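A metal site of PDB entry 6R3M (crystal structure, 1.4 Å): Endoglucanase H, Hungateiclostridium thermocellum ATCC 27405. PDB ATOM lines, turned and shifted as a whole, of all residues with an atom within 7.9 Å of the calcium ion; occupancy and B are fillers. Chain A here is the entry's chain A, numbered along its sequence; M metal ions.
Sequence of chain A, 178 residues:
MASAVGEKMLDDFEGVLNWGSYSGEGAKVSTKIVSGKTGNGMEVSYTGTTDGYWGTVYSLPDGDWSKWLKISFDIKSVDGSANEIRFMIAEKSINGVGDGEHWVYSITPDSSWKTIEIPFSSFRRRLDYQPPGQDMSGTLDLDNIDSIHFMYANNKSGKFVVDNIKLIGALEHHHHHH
The calcium ion is bound by the side-chain carboxylate (OD2) of Asp 141 (2.3 Å), the side-chain carboxylate (OE1) of Glu 101 (2.4 Å), the backbone carbonyl oxygen (O) of Thr 139 (2.4 Å), the side-chain carboxylate (OE1) of Glu 91 (2.5 Å), the side-chain hydroxyl (OG) of Ser 137 (2.5 Å), the side-chain carboxylate (OE2) of Glu 91 (2.5 Å), the side-chain carboxylate (OD2) of Asp 135 (2.5 Å) and the side-chain carboxylate (OD1) of Asp 135 (2.6 Å). The calcium ion has eight donor atoms within binding distance.
Within 4 Å of the calcium ion: Glu 91, Glu 101, Asp 135, Ser 137, Thr 139 and Asp 141. Along chain A the residues within 4 Å of the calcium ion span positions 91 to 141.
The side-chain carboxylate of Glu 101 sits close to the indole nitrogen of Trp 103, at 3.0 Å. The side-chain carboxylate of Glu 101 is in hydrogen-bond range of the backbone NH of Gly 138 (2.9 Å). The side-chain carboxylate (OE2) of Glu 91 sits close to the indole nitrogen (NE1) of Trp 103 (3.5 Å). The backbone carbonyl oxygen of Glu 91 is in hydrogen-bond range of the backbone NH of Gly 100.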
ATOM      1  N   GLU A  91     -13.348   9.893  -7.614  1.00  0.00           N
ATOM      2  CA  GLU A  91     -12.661   9.971  -6.328  1.00  0.00           C
ATOM      3  C   GLU A  91     -12.321   8.573  -5.827  1.00  0.00           C
ATOM      4  O   GLU A  91     -12.870   7.569  -6.317  1.00  0.00           O
ATOM      5  CB  GLU A  91     -13.552  10.690  -5.299  1.00  0.00           C
ATOM      6  CG  GLU A  91     -13.821  12.140  -5.662  1.00  0.00           C
ATOM      7  CD  GLU A  91     -14.775  12.867  -4.699  1.00  0.00           C
ATOM      8  OE1 GLU A  91     -15.292  12.230  -3.747  1.00  0.00           O
ATOM      9  OE2 GLU A  91     -15.093  14.007  -4.965  1.00  0.00           O
ATOM     10  N   LYS A  92     -11.496   8.536  -4.783  1.00  0.00           N
ATOM     11  CA  LYS A  92     -11.226   7.274  -4.110  1.00  0.00           C
ATOM     12  C   LYS A  92     -12.423   6.932  -3.215  1.00  0.00           C
ATOM     13  O   LYS A  92     -13.176   7.809  -2.729  1.00  0.00           O
ATOM     14  CB  LYS A  92      -9.937   7.375  -3.285  1.00  0.00           C
ATOM     15  CG  LYS A  92      -8.670   7.435  -4.110  1.00  0.00           C
ATOM     16  CD  LYS A  92      -7.465   7.840  -3.308  1.00  0.00           C
ATOM     17  CE  LYS A  92      -6.189   7.807  -4.145  1.00  0.00           C
ATOM     18  NZ  LYS A  92      -5.173   8.688  -3.552  1.00  0.00           N
ATOM     19  N   ILE A  94     -14.614   5.561  -0.024  1.00  0.00           N
ATOM     20  CA  ILE A  94     -14.648   5.792   1.455  1.00  0.00           C
ATOM     21  C   ILE A  94     -14.493   4.429   2.185  1.00  0.00           C
ATOM     22  O   ILE A  94     -14.288   4.465   3.360  1.00  0.00           O
ATOM     23  CB  ILE A  94     -15.986   6.425   1.920  1.00  0.00           C
ATOM     24  CG1 ILE A  94     -17.185   5.493   1.743  1.00  0.00           C
ATOM     25  CG2 ILE A  94     -16.280   7.776   1.315  1.00  0.00           C
ATOM     26  CD1 ILE A  94     -18.498   5.996   2.331  1.00  0.00           C
ATOM     27  N   GLY A 100     -14.848   5.876  -5.696  1.00  0.00           N
ATOM     28  CA  GLY A 100     -15.707   6.865  -5.050  1.00  0.00           C
ATOM     29  C   GLY A 100     -16.416   7.731  -6.076  1.00  0.00           C
ATOM     30  O   GLY A 100     -16.581   7.348  -7.246  1.00  0.00           O
ATOM     31  N   GLU A 101     -16.886   8.878  -5.585  1.00  0.00           N
ATOM     32  CA  GLU A 101     -17.812   9.753  -6.308  1.00  0.00           C
ATOM     33  C   GLU A 101     -17.345  10.030  -7.730  1.00  0.00           C
ATOM     34  O   GLU A 101     -16.209  10.422  -7.964  1.00  0.00           O
ATOM     35  CB  GLU A 101     -17.965  11.051  -5.506  1.00  0.00           C
ATOM     36  CG  GLU A 101     -19.227  11.845  -5.859  1.00  0.00           C
ATOM     37  CD  GLU A 101     -19.359  13.065  -4.977  1.00  0.00           C
ATOM     38  OE1 GLU A 101     -18.350  13.723  -4.750  1.00  0.00           O
ATOM     39  OE2 GLU A 101     -20.519  13.397  -4.570  1.00  0.00           O
ATOM     40  N   HIS A 102     -18.282   9.894  -8.687  1.00  0.00           N
ATOM     41  CA  HIS A 102     -18.052  10.100 -10.102  1.00  0.00           C
ATOM     42  C   HIS A 102     -18.455  11.494 -10.550  1.00  0.00           C
ATOM     43  O   HIS A 102     -19.556  11.976 -10.232  1.00  0.00           O
ATOM     44  CB  HIS A 102     -18.898   9.108 -10.925  1.00  0.00           C
ATOM     45  CG  HIS A 102     -18.426   7.706 -10.848  1.00  0.00           C
ATOM     46  ND1 HIS A 102     -19.020   6.694 -11.641  1.00  0.00           N
ATOM     47  CD2 HIS A 102     -17.395   7.132 -10.206  1.00  0.00           C
ATOM     48  CE1 HIS A 102     -18.366   5.557 -11.411  1.00  0.00           C
ATOM     49  NE2 HIS A 102     -17.395   5.789 -10.526  1.00  0.00           N
ATOM     50  N   TRP A 103     -17.537  12.104 -11.307  1.00  0.00           N
ATOM     51  CA  TRP A 103     -17.705  13.472 -11.809  1.00  0.00           C
ATOM     52  C   TRP A 103     -17.460  13.427 -13.314  1.00  0.00           C
ATOM     53  O   TRP A 103     -16.427  12.906 -13.750  1.00  0.00           O
ATOM     54  CB  TRP A 103     -16.694  14.403 -11.105  1.00  0.00           C
ATOM     55  CG  TRP A 103     -17.084  14.612  -9.696  1.00  0.00           C
ATOM     56  CD1 TRP A 103     -16.790  13.797  -8.626  1.00  0.00           C
ATOM     57  CD2 TRP A 103     -17.949  15.645  -9.211  1.00  0.00           C
ATOM     58  NE1 TRP A 103     -17.417  14.286  -7.500  1.00  0.00           N
ATOM     59  CE2 TRP A 103     -18.124  15.420  -7.835  1.00  0.00           C
ATOM     60  CE3 TRP A 103     -18.551  16.773  -9.819  1.00  0.00           C
ATOM     61  CZ2 TRP A 103     -18.946  16.230  -7.051  1.00  0.00           C
ATOM     62  CZ3 TRP A 103     -19.340  17.600  -9.027  1.00  0.00           C
ATOM     63  CH2 TRP A 103     -19.515  17.329  -7.654  1.00  0.00           C
ATOM     64  N   ARG A 125     -21.628  16.408 -11.123  1.00  0.00           N
ATOM     65  CA  ARG A 125     -21.795  15.171 -10.375  1.00  0.00           C
ATOM     66  C   ARG A 125     -22.598  14.193 -11.248  1.00  0.00           C
ATOM     67  O   ARG A 125     -23.654  14.565 -11.827  1.00  0.00           O
ATOM     68  CB  ARG A 125     -22.586  15.481  -9.089  1.00  0.00           C
ATOM     69  CG  ARG A 125     -22.576  14.341  -8.084  1.00  0.00           C
ATOM     70  CD  ARG A 125     -23.572  14.640  -6.974  1.00  0.00           C
ATOM     71  NE  ARG A 125     -24.952  14.437  -7.448  1.00  0.00           N
ATOM     72  CZ  ARG A 125     -25.513  13.227  -7.563  1.00  0.00           C
ATOM     73  NH1 ARG A 125     -24.872  12.110  -7.224  1.00  0.00           N
ATOM     74  NH2 ARG A 125     -26.752  13.127  -8.017  1.00  0.00           N
ATOM     75  N   GLN A 134     -18.858   5.894  -2.812  1.00  0.00           N
ATOM     76  CA  GLN A 134     -18.886   7.361  -2.963  1.00  0.00           C
ATOM     77  C   GLN A 134     -19.095   8.036  -1.605  1.00  0.00           C
ATOM     78  O   GLN A 134     -19.764   7.486  -0.754  1.00  0.00           O
ATOM     79  CB  GLN A 134     -19.983   7.779  -3.953  1.00  0.00           C
ATOM     80  CG  GLN A 134     -21.425   7.482  -3.472  1.00  0.00           C
ATOM     81  CD  GLN A 134     -22.402   8.569  -3.883  1.00  0.00           C
ATOM     82  OE1 GLN A 134     -23.566   8.314  -4.125  1.00  0.00           O
ATOM     83  NE2 GLN A 134     -21.885   9.766  -3.972  1.00  0.00           N
ATOM     84  N   ASP A 135     -18.582   9.253  -1.513  1.00  0.00           N
ATOM     85  CA  ASP A 135     -18.691  10.056  -0.265  1.00  0.00           C
ATOM     86  C   ASP A 135     -20.014  10.799  -0.198  1.00  0.00           C
ATOM     87  O   ASP A 135     -20.323  11.292   0.826  1.00  0.00           O
ATOM     88  CB  ASP A 135     -17.482  10.995  -0.113  1.00  0.00           C
ATOM     89  CG  ASP A 135     -17.351  12.166  -1.091  1.00  0.00           C
ATOM     90  OD1 ASP A 135     -18.145  12.271  -1.991  1.00  0.00           O
ATOM     91  OD2 ASP A 135     -16.438  12.902  -0.947  1.00  0.00           O
ATOM     92  N   MET A 136     -20.797  10.801  -1.258  1.00  0.00           N
ATOM     93  CA  MET A 136     -22.005  11.596  -1.330  1.00  0.00           C
ATOM     94  C   MET A 136     -21.799  13.053  -0.886  1.00  0.00           C
ATOM     95  O   MET A 136     -22.722  13.676  -0.362  1.00  0.00           O
ATOM     96  CB  MET A 136     -23.147  11.002  -0.479  1.00  0.00           C
ATOM     97  CG  MET A 136     -23.717   9.747  -1.078  1.00  0.00           C
ATOM     98  SD  MET A 136     -25.157   9.090  -0.147  1.00  0.00           S
ATOM     99  CE  MET A 136     -24.288   8.663   1.346  1.00  0.00           C
ATOM    100  N   SER A 137     -20.626  13.632  -1.160  1.00  0.00           N
ATOM    101  CA  SER A 137     -20.330  14.993  -0.693  1.00  0.00           C
ATOM    102  C   SER A 137     -20.943  16.046  -1.623  1.00  0.00           C
ATOM    103  O   SER A 137     -21.202  17.175  -1.208  1.00  0.00           O
ATOM    104  CB  SER A 137     -18.850  15.254  -0.499  1.00  0.00           C
ATOM    105  OG  SER A 137     -18.179  15.549  -1.730  1.00  0.00           O
ATOM    106  N   GLY A 138     -21.153  15.689  -2.895  1.00  0.00           N
ATOM    107  CA  GLY A 138     -21.567  16.608  -3.943  1.00  0.00           C
ATOM    108  C   GLY A 138     -20.538  17.678  -4.261  1.00  0.00           C
ATOM    109  O   GLY A 138     -20.842  18.689  -4.908  1.00  0.00           O
ATOM    110  N   THR A 139     -19.279  17.417  -3.891  1.00  0.00           N
ATOM    111  CA  THR A 139     -18.162  18.275  -4.269  1.00  0.00           C
ATOM    112  C   THR A 139     -17.026  17.377  -4.725  1.00  0.00           C
ATOM    113  O   THR A 139     -16.780  16.343  -4.127  1.00  0.00           O
ATOM    114  CB  THR A 139     -17.672  19.102  -3.081  1.00  0.00           C
ATOM    115  OG1 THR A 139     -17.343  18.171  -2.051  1.00  0.00           O
ATOM    116  CG2 THR A 139     -18.762  20.030  -2.578  1.00  0.00           C
ATOM    117  N   LEU A 140     -16.355  17.800  -5.785  1.00  0.00           N
ATOM    118  CA  LEU A 140     -15.190  17.073  -6.289  1.00  0.00           C
ATOM    119  C   LEU A 140     -14.013  17.364  -5.378  1.00  0.00           C
ATOM    120  O   LEU A 140     -13.573  18.514  -5.267  1.00  0.00           O
ATOM    121  CB  LEU A 140     -14.906  17.541  -7.720  1.00  0.00           C
ATOM    122  CG  LEU A 140     -13.662  16.979  -8.401  1.00  0.00           C
ATOM    123  CD1 LEU A 140     -13.589  15.450  -8.349  1.00  0.00           C
ATOM    124  CD2 LEU A 140     -13.601  17.449  -9.849  1.00  0.00           C
ATOM    125  N   ASP A 141     -13.508  16.319  -4.722  1.00  0.00           N
ATOM    126  CA  ASP A 141     -12.459  16.496  -3.732  1.00  0.00           C
ATOM    127  C   ASP A 141     -11.117  16.212  -4.401  1.00  0.00           C
ATOM    128  O   ASP A 141     -10.745  15.046  -4.562  1.00  0.00           O
ATOM    129  CB  ASP A 141     -12.714  15.517  -2.572  1.00  0.00           C
ATOM    130  CG  ASP A 141     -14.005  15.880  -1.865  1.00  0.00           C
ATOM    131  OD1 ASP A 141     -13.984  16.924  -1.181  1.00  0.00           O
ATOM    132  OD2 ASP A 141     -15.002  15.147  -1.953  1.00  0.00           O
ATOM    133  N   LEU A 142     -10.411  17.300  -4.805  1.00  0.00           N
ATOM    134  CA  LEU A 142      -9.247  17.173  -5.659  1.00  0.00           C
ATOM    135  C   LEU A 142      -8.048  16.554  -4.922  1.00  0.00           C
ATOM    136  O   LEU A 142      -7.089  16.184  -5.586  1.00  0.00           O
ATOM    137  CB  LEU A 142      -8.905  18.544  -6.243  1.00  0.00           C
ATOM    138  CG  LEU A 142      -9.926  18.988  -7.293  1.00  0.00           C
ATOM    139  CD1 LEU A 142      -9.739  20.470  -7.604  1.00  0.00           C
ATOM    140  CD2 LEU A 142      -9.796  18.166  -8.577  1.00  0.00           C
ATOM    141  N   ASN A 144      -8.185  13.711  -3.510  1.00  0.00           N
ATOM    142  CA  ASN A 144      -8.627  12.343  -3.283  1.00  0.00           C
ATOM    143  C   ASN A 144      -9.061  11.679  -4.588  1.00  0.00           C
ATOM    144  O   ASN A 144     -10.102  11.019  -4.634  1.00  0.00           O
ATOM    145  CB  ASN A 144      -9.739  12.283  -2.227  1.00  0.00           C
ATOM    146  CG  ASN A 144      -9.768  10.933  -1.527  1.00  0.00           C
ATOM    147  OD1 ASN A 144      -8.703  10.382  -1.205  1.00  0.00           O
ATOM    148  ND2 ASN A 144     -10.964  10.416  -1.291  1.00  0.00           N
HETATM  149 CA    CA M   1     -16.702  14.129  -3.090  1.00  0.00          CA
